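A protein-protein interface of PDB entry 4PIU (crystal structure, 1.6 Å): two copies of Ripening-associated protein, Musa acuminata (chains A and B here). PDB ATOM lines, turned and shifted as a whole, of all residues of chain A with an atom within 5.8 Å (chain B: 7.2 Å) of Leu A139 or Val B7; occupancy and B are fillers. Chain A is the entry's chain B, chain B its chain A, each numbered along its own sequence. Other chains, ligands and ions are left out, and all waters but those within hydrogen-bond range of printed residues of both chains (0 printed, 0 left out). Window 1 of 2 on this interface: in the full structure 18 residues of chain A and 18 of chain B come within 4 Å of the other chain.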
ATOM      1  N   ALA A   4      13.523 -19.013   8.486  1.00  0.00           N
ATOM      2  CA  ALA A   4      12.508 -18.740   9.533  1.00  0.00           C
ATOM      3  C   ALA A   4      13.046 -17.924  10.700  1.00  0.00           C
ATOM      4  O   ALA A   4      14.221 -18.058  11.066  1.00  0.00           O
ATOM      5  CB  ALA A   4      11.939 -20.067  10.041  1.00  0.00           C
ATOM      6  N   ILE A   5      12.198 -17.060  11.250  1.00  0.00           N
ATOM      7  CA  ILE A   5      12.461 -16.430  12.552  1.00  0.00           C
ATOM      8  C   ILE A   5      11.352 -16.882  13.499  1.00  0.00           C
ATOM      9  O   ILE A   5      10.152 -16.623  13.255  1.00  0.00           O
ATOM     10  CB  ILE A   5      12.527 -14.871  12.440  1.00  0.00           C
ATOM     11  CG1 ILE A   5      13.703 -14.446  11.540  1.00  0.00           C
ATOM     12  CG2 ILE A   5      12.639 -14.250  13.847  1.00  0.00           C
ATOM     13  CD1 ILE A   5      13.864 -12.938  11.292  1.00  0.00           C
ATOM     14  N   LYS A   6      11.743 -17.547  14.578  1.00  0.00           N
ATOM     15  CA  LYS A   6      10.760 -18.056  15.551  1.00  0.00           C
ATOM     16  C   LYS A   6      11.128 -17.525  16.921  1.00  0.00           C
ATOM     17  O   LYS A   6      12.275 -17.662  17.336  1.00  0.00           O
ATOM     18  CB  LYS A   6      10.850 -19.593  15.617  1.00  0.00           C
ATOM     19  CG  LYS A   6      10.330 -20.306  14.373  1.00  0.00           C
ATOM     20  CD  LYS A   6      10.681 -21.813  14.342  1.00  0.00           C
ATOM     21  CE  LYS A   6       9.784 -22.660  15.256  1.00  0.00           C
ATOM     22  NZ  LYS A   6      10.237 -24.083  15.105  1.00  0.00           N
ATOM     23  N   VAL A   7      10.179 -16.862  17.577  1.00  0.00           N
ATOM     24  CA  VAL A   7      10.411 -16.352  18.944  1.00  0.00           C
ATOM     25  C   VAL A   7       9.443 -17.017  19.916  1.00  0.00           C
ATOM     26  O   VAL A   7       8.303 -17.381  19.550  1.00  0.00           O
ATOM     27  CB  VAL A   7      10.288 -14.813  19.017  1.00  0.00           C
ATOM     28  CG1 VAL A   7      11.410 -14.195  18.167  1.00  0.00           C
ATOM     29  CG2 VAL A   7       8.904 -14.282  18.532  1.00  0.00           C
ATOM     30  N   LEU A 114       5.161  -9.312  23.567  1.00  0.00           N
ATOM     31  CA  LEU A 114       5.872  -9.259  22.312  1.00  0.00           C
ATOM     32  C   LEU A 114       5.271  -8.138  21.485  1.00  0.00           C
ATOM     33  O   LEU A 114       4.405  -8.368  20.634  1.00  0.00           O
ATOM     34  CB  LEU A 114       5.810 -10.627  21.604  1.00  0.00           C
ATOM     35  CG  LEU A 114       6.583 -10.639  20.276  1.00  0.00           C
ATOM     36  CD1 LEU A 114       8.110 -10.749  20.516  1.00  0.00           C
ATOM     37  CD2 LEU A 114       6.094 -11.835  19.394  1.00  0.00           C
ATOM     38  N   PRO A 115       5.746  -6.904  21.703  1.00  0.00           N
ATOM     39  CA  PRO A 115       5.408  -5.824  20.760  1.00  0.00           C
ATOM     40  C   PRO A 115       6.226  -6.028  19.476  1.00  0.00           C
ATOM     41  O   PRO A 115       7.419  -6.323  19.564  1.00  0.00           O
ATOM     42  CB  PRO A 115       5.879  -4.546  21.494  1.00  0.00           C
ATOM     43  CG  PRO A 115       6.556  -4.962  22.714  1.00  0.00           C
ATOM     44  CD  PRO A 115       6.683  -6.475  22.759  1.00  0.00           C
ATOM     45  N   ILE A 116       5.598  -5.959  18.316  1.00  0.00           N
ATOM     46  CA  ILE A 116       6.336  -6.072  17.048  1.00  0.00           C
ATOM     47  C   ILE A 116       6.331  -4.702  16.379  1.00  0.00           C
ATOM     48  O   ILE A 116       5.293  -4.279  15.831  1.00  0.00           O
ATOM     49  CB  ILE A 116       5.737  -7.161  16.139  1.00  0.00           C
ATOM     50  CG1 ILE A 116       5.666  -8.500  16.893  1.00  0.00           C
ATOM     51  CG2 ILE A 116       6.601  -7.346  14.844  1.00  0.00           C
ATOM     52  CD1 ILE A 116       4.729  -9.567  16.263  1.00  0.00           C
ATOM     53  N   ALA A 117       7.467  -3.994  16.462  1.00  0.00           N
ATOM     54  CA  ALA A 117       7.630  -2.668  15.858  1.00  0.00           C
ATOM     55  C   ALA A 117       7.661  -2.698  14.328  1.00  0.00           C
ATOM     56  O   ALA A 117       7.188  -1.756  13.656  1.00  0.00           O
ATOM     57  CB  ALA A 117       8.903  -1.991  16.388  1.00  0.00           C
ATOM     58  N   ALA A 118       8.240  -3.766  13.784  1.00  0.00           N
ATOM     59  CA  ALA A 118       8.229  -3.992  12.349  1.00  0.00           C
ATOM     60  C   ALA A 118       8.125  -5.481  12.114  1.00  0.00           C
ATOM     61  O   ALA A 118       8.904  -6.267  12.651  1.00  0.00           O
ATOM     62  CB  ALA A 118       9.491  -3.445  11.738  1.00  0.00           C
ATOM     63  N   LYS A 120       5.198  -8.994  11.363  1.00  0.00           N
ATOM     64  CA  LYS A 120       3.900  -9.582  11.737  1.00  0.00           C
ATOM     65  C   LYS A 120       4.065 -11.034  12.058  1.00  0.00           C
ATOM     66  O   LYS A 120       5.063 -11.663  11.669  1.00  0.00           O
ATOM     67  CB  LYS A 120       2.870  -9.395  10.614  1.00  0.00           C
ATOM     68  CG  LYS A 120       3.122 -10.199   9.363  1.00  0.00           C
ATOM     69  CD  LYS A 120       1.982  -9.930   8.349  1.00  0.00           C
ATOM     70  CE  LYS A 120       2.309 -10.679   7.057  1.00  0.00           C
ATOM     71  NZ  LYS A 120       1.159 -10.757   6.114  1.00  0.00           N
ATOM     72  N   ILE A 121       3.090 -11.571  12.799  1.00  0.00           N
ATOM     73  CA  ILE A 121       3.046 -13.006  13.074  1.00  0.00           C
ATOM     74  C   ILE A 121       2.545 -13.763  11.857  1.00  0.00           C
ATOM     75  O   ILE A 121       1.526 -13.408  11.268  1.00  0.00           O
ATOM     76  CB  ILE A 121       2.135 -13.274  14.281  1.00  0.00           C
ATOM     77  CG1 ILE A 121       2.791 -12.653  15.521  1.00  0.00           C
ATOM     78  CG2 ILE A 121       1.785 -14.766  14.431  1.00  0.00           C
ATOM     79  CD1 ILE A 121       1.854 -12.515  16.770  1.00  0.00           C
ATOM     80  N   SER A 122       3.274 -14.820  11.493  1.00  0.00           N
ATOM     81  CA  SER A 122       2.904 -15.597  10.305  1.00  0.00           C
ATOM     82  C   SER A 122       2.623 -17.074  10.583  1.00  0.00           C
ATOM     83  O   SER A 122       2.254 -17.812   9.666  1.00  0.00           O
ATOM     84  CB  SER A 122       4.020 -15.475   9.263  1.00  0.00           C
ATOM     85  OG  SER A 122       5.239 -15.954   9.831  1.00  0.00           O
ATOM     86  N   GLY A 123       2.726 -17.499  11.837  1.00  0.00           N
ATOM     87  CA  GLY A 123       2.461 -18.899  12.160  1.00  0.00           C
ATOM     88  C   GLY A 123       2.729 -19.126  13.630  1.00  0.00           C
ATOM     89  O   GLY A 123       3.216 -18.232  14.323  1.00  0.00           O
ATOM     90  N   VAL A 137       5.749 -17.836  18.151  1.00  0.00           N
ATOM     91  CA  VAL A 137       5.321 -17.390  16.819  1.00  0.00           C
ATOM     92  C   VAL A 137       6.461 -17.331  15.808  1.00  0.00           C
ATOM     93  O   VAL A 137       7.647 -17.122  16.179  1.00  0.00           O
ATOM     94  CB  VAL A 137       4.640 -16.003  16.864  1.00  0.00           C
ATOM     95  CG1 VAL A 137       3.309 -16.084  17.616  1.00  0.00           C
ATOM     96  CG2 VAL A 137       5.557 -14.943  17.520  1.00  0.00           C
ATOM     97  N   TYR A 138       6.081 -17.550  14.554  1.00  0.00           N
ATOM     98  CA  TYR A 138       6.911 -17.192  13.385  1.00  0.00           C
ATOM     99  C   TYR A 138       6.667 -15.749  13.045  1.00  0.00           C
ATOM    100  O   TYR A 138       5.549 -15.252  13.158  1.00  0.00           O
ATOM    101  CB  TYR A 138       6.510 -18.021  12.175  1.00  0.00           C
ATOM    102  CG  TYR A 138       6.933 -19.459  12.249  1.00  0.00           C
ATOM    103  CD1 TYR A 138       6.203 -20.380  13.006  1.00  0.00           C
ATOM    104  CD2 TYR A 138       8.046 -19.895  11.552  1.00  0.00           C
ATOM    105  CE1 TYR A 138       6.573 -21.738  13.065  1.00  0.00           C
ATOM    106  CE2 TYR A 138       8.452 -21.247  11.596  1.00  0.00           C
ATOM    107  CZ  TYR A 138       7.697 -22.169  12.342  1.00  0.00           C
ATOM    108  OH  TYR A 138       8.112 -23.488  12.395  1.00  0.00           O
ATOM    109  N   LEU A 139       7.736 -15.075  12.623  1.00  0.00           N
ATOM    110  CA  LEU A 139       7.640 -13.672  12.198  1.00  0.00           C
ATOM    111  C   LEU A 139       8.043 -13.503  10.736  1.00  0.00           C
ATOM    112  O   LEU A 139       8.872 -14.247  10.192  1.00  0.00           O
ATOM    113  CB  LEU A 139       8.557 -12.764  13.044  1.00  0.00           C
ATOM    114  CG  LEU A 139       8.273 -12.828  14.547  1.00  0.00           C
ATOM    115  CD1 LEU A 139       9.316 -11.984  15.300  1.00  0.00           C
ATOM    116  CD2 LEU A 139       6.852 -12.293  14.890  1.00  0.00           C
ATOM    117  N   GLU A 140       7.475 -12.483  10.114  1.00  0.00           N
ATOM    118  CA  GLU A 140       7.889 -12.086   8.764  1.00  0.00           C
ATOM    119  C   GLU A 140       7.658 -10.584   8.584  1.00  0.00           C
ATOM    120  O   GLU A 140       6.971  -9.964   9.380  1.00  0.00           O
ATOM    121  CB  GLU A 140       7.155 -12.932   7.704  1.00  0.00           C
ATOM    122  CG  GLU A 140       5.896 -12.324   7.171  1.00  0.00           C
ATOM    123  CD  GLU A 140       5.327 -13.137   6.031  1.00  0.00           C
ATOM    124  OE1 GLU A 140       5.737 -14.300   5.849  1.00  0.00           O
ATOM    125  OE2 GLU A 140       4.476 -12.614   5.316  1.00  0.00           O
ATOM    126  N   PRO A 141       8.247  -9.985   7.530  1.00  0.00           N
ATOM    127  CA  PRO A 141       8.087  -8.531   7.333  1.00  0.00           C
ATOM    128  C   PRO A 141       6.658  -8.077   7.097  1.00  0.00           C
ATOM    129  O   PRO A 141       5.802  -8.854   6.613  1.00  0.00           O
ATOM    130  CB  PRO A 141       8.912  -8.257   6.066  1.00  0.00           C
ATOM    131  CG  PRO A 141       9.988  -9.379   6.130  1.00  0.00           C
ATOM    132  CD  PRO A 141       9.203 -10.565   6.571  1.00  0.00           C
ATOM    133  N   ILE B   5      12.635  -6.909  10.683  1.00  0.00           N
ATOM    134  CA  ILE B   5      11.957  -7.515  11.837  1.00  0.00           C
ATOM    135  C   ILE B   5      12.448  -6.867  13.116  1.00  0.00           C
ATOM    136  O   ILE B   5      13.618  -7.060  13.524  1.00  0.00           O
ATOM    137  CB  ILE B   5      12.190  -9.069  11.942  1.00  0.00           C
ATOM    138  CG1 ILE B   5      11.841  -9.783  10.619  1.00  0.00           C
ATOM    139  CG2 ILE B   5      11.387  -9.626  13.147  1.00  0.00           C
ATOM    140  CD1 ILE B   5      10.374  -9.669  10.242  1.00  0.00           C
ATOM    141  N   LYS B   6      11.577  -6.068  13.736  1.00  0.00           N
ATOM    142  CA  LYS B   6      11.959  -5.346  14.973  1.00  0.00           C
ATOM    143  C   LYS B   6      10.970  -5.706  16.046  1.00  0.00           C
ATOM    144  O   LYS B   6       9.766  -5.598  15.837  1.00  0.00           O
ATOM    145  CB  LYS B   6      11.904  -3.832  14.743  1.00  0.00           C
ATOM    146  CG  LYS B   6      13.007  -3.316  13.793  1.00  0.00           C
ATOM    147  CD  LYS B   6      12.752  -1.883  13.379  1.00  0.00           C
ATOM    148  CE  LYS B   6      13.076  -0.903  14.523  1.00  0.00           C
ATOM    149  NZ  LYS B   6      13.017   0.525  14.035  1.00  0.00           N
ATOM    150  N   VAL B   7      11.461  -6.181  17.196  1.00  0.00           N
ATOM    151  CA  VAL B   7      10.556  -6.581  18.293  1.00  0.00           C
ATOM    152  C   VAL B   7      10.953  -5.771  19.508  1.00  0.00           C
ATOM    153  O   VAL B   7      12.128  -5.422  19.679  1.00  0.00           O
ATOM    154  CB  VAL B   7      10.546  -8.113  18.562  1.00  0.00           C
ATOM    155  CG1 VAL B   7      10.019  -8.854  17.309  1.00  0.00           C
ATOM    156  CG2 VAL B   7      11.910  -8.651  18.960  1.00  0.00           C
ATOM    157  N   GLY B   8       9.977  -5.462  20.367  1.00  0.00           N
ATOM    158  CA  GLY B   8      10.231  -4.455  21.392  1.00  0.00           C
ATOM    159  C   GLY B   8       9.710  -3.105  20.863  1.00  0.00           C
ATOM    160  O   GLY B   8       8.959  -3.059  19.883  1.00  0.00           O
ATOM    161  N   ALA B   9      10.097  -1.994  21.485  1.00  0.00           N
ATOM    162  CA  ALA B   9      10.985  -1.986  22.631  1.00  0.00           C
ATOM    163  C   ALA B   9      10.213  -2.266  23.929  1.00  0.00           C
ATOM    164  O   ALA B   9       8.980  -2.040  24.020  1.00  0.00           O
ATOM    165  CB  ALA B   9      11.709  -0.583  22.714  1.00  0.00           C
ATOM    166  N   TRP B  10      10.950  -2.792  24.908  1.00  0.00           N
ATOM    167  CA  TRP B  10      10.442  -2.918  26.277  1.00  0.00           C
ATOM    168  C   TRP B  10      11.030  -1.781  27.109  1.00  0.00           C
ATOM    169  O   TRP B  10      12.237  -1.517  27.023  1.00  0.00           O
ATOM    170  CB  TRP B  10      10.912  -4.265  26.852  1.00  0.00           C
ATOM    171  CG  TRP B  10      10.242  -5.410  26.186  1.00  0.00           C
ATOM    172  CD1 TRP B  10       9.045  -5.974  26.535  1.00  0.00           C
ATOM    173  CD2 TRP B  10      10.737  -6.164  25.071  1.00  0.00           C
ATOM    174  NE1 TRP B  10       8.745  -7.015  25.684  1.00  0.00           N
ATOM    175  CE2 TRP B  10       9.776  -7.153  24.780  1.00  0.00           C
ATOM    176  CE3 TRP B  10      11.905  -6.088  24.278  1.00  0.00           C
ATOM    177  CZ2 TRP B  10       9.942  -8.078  23.740  1.00  0.00           C
ATOM    178  CZ3 TRP B  10      12.070  -7.001  23.250  1.00  0.00           C
ATOM    179  CH2 TRP B  10      11.088  -7.991  22.984  1.00  0.00           C
ATOM    180  N   MET B  76      17.108 -12.280  24.858  1.00  0.00           N
ATOM    181  CA  MET B  76      17.241 -11.092  25.699  1.00  0.00           C
ATOM    182  C   MET B  76      16.091 -11.155  26.698  1.00  0.00           C
ATOM    183  O   MET B  76      14.996 -11.596  26.343  1.00  0.00           O
ATOM    184  CB  MET B  76      17.148  -9.823  24.845  1.00  0.00           C
ATOM    185  CG  MET B  76      17.372  -8.535  25.672  1.00  0.00           C
ATOM    186  SD  MET B  76      17.399  -7.018  24.623  1.00  0.00           S
ATOM    187  CE  MET B  76      15.663  -6.928  24.135  1.00  0.00           C
ATOM    188  N   LEU B 114      12.590 -12.667  25.780  1.00  0.00           N
ATOM    189  CA  LEU B 114      12.560 -12.975  24.349  1.00  0.00           C
ATOM    190  C   LEU B 114      13.484 -14.142  24.034  1.00  0.00           C
ATOM    191  O   LEU B 114      14.645 -13.941  23.670  1.00  0.00           O
ATOM    192  CB  LEU B 114      12.973 -11.724  23.527  1.00  0.00           C
ATOM    193  CG  LEU B 114      12.904 -11.940  22.014  1.00  0.00           C
ATOM    194  CD1 LEU B 114      11.431 -11.866  21.556  1.00  0.00           C
ATOM    195  CD2 LEU B 114      13.765 -10.869  21.322  1.00  0.00           C
ATOM    196  N   ILE B 116      14.740 -16.781  21.402  1.00  0.00           N
ATOM    197  CA  ILE B 116      14.707 -16.873  19.931  1.00  0.00           C
ATOM    198  C   ILE B 116      14.966 -18.331  19.549  1.00  0.00           C
ATOM    199  O   ILE B 116      16.105 -18.801  19.627  1.00  0.00           O
ATOM    200  CB  ILE B 116      15.724 -15.928  19.311  1.00  0.00           C
ATOM    201  CG1 ILE B 116      15.447 -14.499  19.824  1.00  0.00           C
ATOM    202  CG2 ILE B 116      15.649 -16.025  17.760  1.00  0.00           C
ATOM    203  CD1 ILE B 116      16.574 -13.535  19.623  1.00  0.00           C
ATOM    204  N   ILE B 121      19.790 -12.063  17.234  1.00  0.00           N
ATOM    205  CA  ILE B 121      19.734 -10.592  17.382  1.00  0.00           C
ATOM    206  C   ILE B 121      20.867  -9.994  16.562  1.00  0.00           C
ATOM    207  O   ILE B 121      22.032 -10.413  16.673  1.00  0.00           O
ATOM    208  CB  ILE B 121      19.877 -10.189  18.869  1.00  0.00           C
ATOM    209  CG1 ILE B 121      18.623 -10.594  19.631  1.00  0.00           C
ATOM    210  CG2 ILE B 121      20.153  -8.664  19.002  1.00  0.00           C
ATOM    211  CD1 ILE B 121      18.889 -10.577  21.158  1.00  0.00           C
ATOM    212  N   PHE B 125      17.423  -1.017  19.045  1.00  0.00           N
ATOM    213  CA  PHE B 125      16.821   0.316  19.012  1.00  0.00           C
ATOM    214  C   PHE B 125      16.185   0.541  20.382  1.00  0.00           C
ATOM    215  O   PHE B 125      16.106  -0.387  21.233  1.00  0.00           O
ATOM    216  CB  PHE B 125      15.754   0.433  17.890  1.00  0.00           C
ATOM    217  CG  PHE B 125      14.548  -0.487  18.070  1.00  0.00           C
ATOM    218  CD1 PHE B 125      13.326   0.015  18.566  1.00  0.00           C
ATOM    219  CD2 PHE B 125      14.649  -1.844  17.728  1.00  0.00           C
ATOM    220  CE1 PHE B 125      12.196  -0.850  18.711  1.00  0.00           C
ATOM    221  CE2 PHE B 125      13.555  -2.713  17.887  1.00  0.00           C
ATOM    222  CZ  PHE B 125      12.339  -2.213  18.366  1.00  0.00           C
ATOM    223  N   ILE B 135      14.503  -0.751  25.296  1.00  0.00           N
ATOM    224  CA  ILE B 135      15.344  -1.459  24.347  1.00  0.00           C
ATOM    225  C   ILE B 135      14.523  -2.489  23.575  1.00  0.00           C
ATOM    226  O   ILE B 135      13.665  -3.184  24.149  1.00  0.00           O
ATOM    227  CB  ILE B 135      16.581  -2.127  25.080  1.00  0.00           C
ATOM    228  CG1 ILE B 135      17.603  -2.600  24.021  1.00  0.00           C
ATOM    229  CG2 ILE B 135      16.118  -3.202  26.053  1.00  0.00           C
ATOM    230  CD1 ILE B 135      19.000  -2.871  24.601  1.00  0.00           C
ATOM    231  N   GLY B 136      14.817  -2.582  22.283  1.00  0.00           N
ATOM    232  CA  GLY B 136      14.249  -3.619  21.417  1.00  0.00           C
ATOM    233  C   GLY B 136      15.350  -4.115  20.492  1.00  0.00           C
ATOM    234  O   GLY B 136      16.489  -3.612  20.515  1.00  0.00           O
ATOM    235  N   VAL B 137      15.032  -5.132  19.696  1.00  0.00           N
ATOM    236  CA  VAL B 137      16.072  -5.767  18.870  1.00  0.00           C
ATOM    237  C   VAL B 137      15.602  -5.959  17.433  1.00  0.00           C
ATOM    238  O   VAL B 137      14.392  -6.144  17.165  1.00  0.00           O
ATOM    239  CB  VAL B 137      16.534  -7.138  19.428  1.00  0.00           C
ATOM    240  CG1 VAL B 137      17.311  -6.989  20.763  1.00  0.00           C
ATOM    241  CG2 VAL B 137      15.322  -8.089  19.619  1.00  0.00           C
ATOM    242  N   TYR B 138      16.570  -5.893  16.528  1.00  0.00           N
ATOM    243  CA  TYR B 138      16.421  -6.431  15.170  1.00  0.00           C
ATOM    244  C   TYR B 138      16.723  -7.919  15.147  1.00  0.00           C
ATOM    245  O   TYR B 138      17.689  -8.379  15.779  1.00  0.00           O
ATOM    246  CB  TYR B 138      17.399  -5.747  14.222  1.00  0.00           C
ATOM    247  CG  TYR B 138      17.044  -4.312  13.896  1.00  0.00           C
ATOM    248  CD1 TYR B 138      17.432  -3.277  14.730  1.00  0.00           C
ATOM    249  CD2 TYR B 138      16.395  -4.009  12.703  1.00  0.00           C
ATOM    250  CE1 TYR B 138      17.082  -1.935  14.419  1.00  0.00           C
ATOM    251  CE2 TYR B 138      16.083  -2.706  12.372  1.00  0.00           C
ATOM    252  CZ  TYR B 138      16.448  -1.683  13.224  1.00  0.00           C
ATOM    253  OH  TYR B 138      16.125  -0.390  12.865  1.00  0.00           O
ATOM    254  N   LEU B 139      15.867  -8.678  14.446  1.00  0.00           N
ATOM    255  CA  LEU B 139      16.059 -10.115  14.291  1.00  0.00           C
ATOM    256  C   LEU B 139      16.355 -10.497  12.853  1.00  0.00           C
ATOM    257  O   LEU B 139      15.782  -9.917  11.900  1.00  0.00           O
ATOM    258  CB  LEU B 139      14.814 -10.868  14.761  1.00  0.00           C
ATOM    259  CG  LEU B 139      14.442 -10.615  16.219  1.00  0.00           C
ATOM    260  CD1 LEU B 139      13.150 -11.385  16.485  1.00  0.00           C
ATOM    261  CD2 LEU B 139      15.555 -11.002  17.185  1.00  0.00           C
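The backbone NH (N) of Lys B6 sits at hydrogen-bond distance from the backbone carbonyl oxygen (O) of Ala A118 (2.9 Å). The backbone NH of Gly B8 sits at hydrogen-bond distance from the backbone carbonyl oxygen of Pro A115 (2.8 Å). The backbone NH (N) of Ala A117 sits at hydrogen-bond distance from the backbone carbonyl oxygen (O) of Lys B6, at 2.9 Å.
The backbone carbonyl oxygen (O) of Met B76 sits at hydrogen-bond distance from the backbone NH (N) of Leu B114 (2.7 Å). N of Val B137 sits at hydrogen-bond distance from O of Val B7, 2.9 Å away. N of Leu A139 sits at hydrogen-bond distance from O of Ile A5, at 2.9 Å. O of Ile B135 sits at hydrogen-bond distance from N of Trp B10. The side-chain carboxylate (OE2) of Glu A140 is in salt-bridge range of the side-chain amino group (NZ) of Lys A120, 3.9 Å away. NZ of Lys A6 lies close to OH of Tyr A138, 3.5 Å away.
Among the printed residues, pairs that only touch across the chains: Ile A5 with Ile B5 (3.8 Å), Ile A5 with Leu B139 (3.6 Å), Lys A6 with Ile B116 (3.5 Å), Val A7 with Leu B139 (3.7 Å), Leu A114 with Leu B114 (3.7 Å), Pro A115 with Val B7 (3.4 Å), Pro A115 with Trp B10 (3.6 Å), Ile A116 with Lys B6 (3.6 Å), Ala A117 with Gly B8 (3.7 Å), Ala A117 with Phe B125 (3.97 Å), Ala A118 with Ile B5 (3.4 Å), Leu A139 with Ile B5 (3.8 Å), Leu A139 with Val B7 (3.8 Å), Glu A140 with Ile B5 (3.3 Å) and Pro A141 with Ile B5 (3.5 Å).
Leu A139 touches just these residues of chain B: Ile B5 (3.8 Å) and Val B7 (3.8 Å). Printed residues of chain B within 4 Å of Ala A117: Lys B6, Gly B8 and Phe B125. Of the printed residues of chain B, Pro A115 touches Val B7 (3.4 Å), Gly B8 (2.8 Å) and Trp B10 (3.6 Å). Of the printed residues of chain B, Leu A114 touches Leu B114. Val A137 touches none of the printed residues of chain B. The nearest residue of chain B that does not touch Leu A139 is Leu B139 (4.1 Å). The nearest residue of chain A that does not touch Val B7 is Leu A114 (4.1 Å).
Hydrophobic or aromatic side chains of chain B that line the printed part of chain A: Ile B5, Val B7, Trp B10, Leu B114, Ile B116, Phe B125 and Leu B139. Hydrophobic or aromatic side chains of chain A that line the printed part of chain B: Ile A5, Val A7, Leu A114, Pro A115, Ile A116, Ala A117, Ala A118, Leu A139 and Pro A141. Along chain A the printed residues that touch a printed residue of chain B span positions 5 to 141. Among the printed residues, 18 pairs touch across the chains. Among the printed residues, no Asp or Glu carboxylate lies within 4 Å of a Lys or Arg side-chain nitrogen of the other chain.
Ile A5 touches Leu B139, and with the chains exchanged Leu A139 touches Ile B5. Lys A6 touches Ile B116, and with the chains exchanged Ile A116 touches Lys B6. Val A7 touches Leu B139, and with the chains exchanged Leu A139 touches Val B7. Leu B114 touches its own counterpart, Leu A114. Of the 18 pairs that touch across the chains among the printed residues, 8 have their exchanged pair printed and touching as well.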
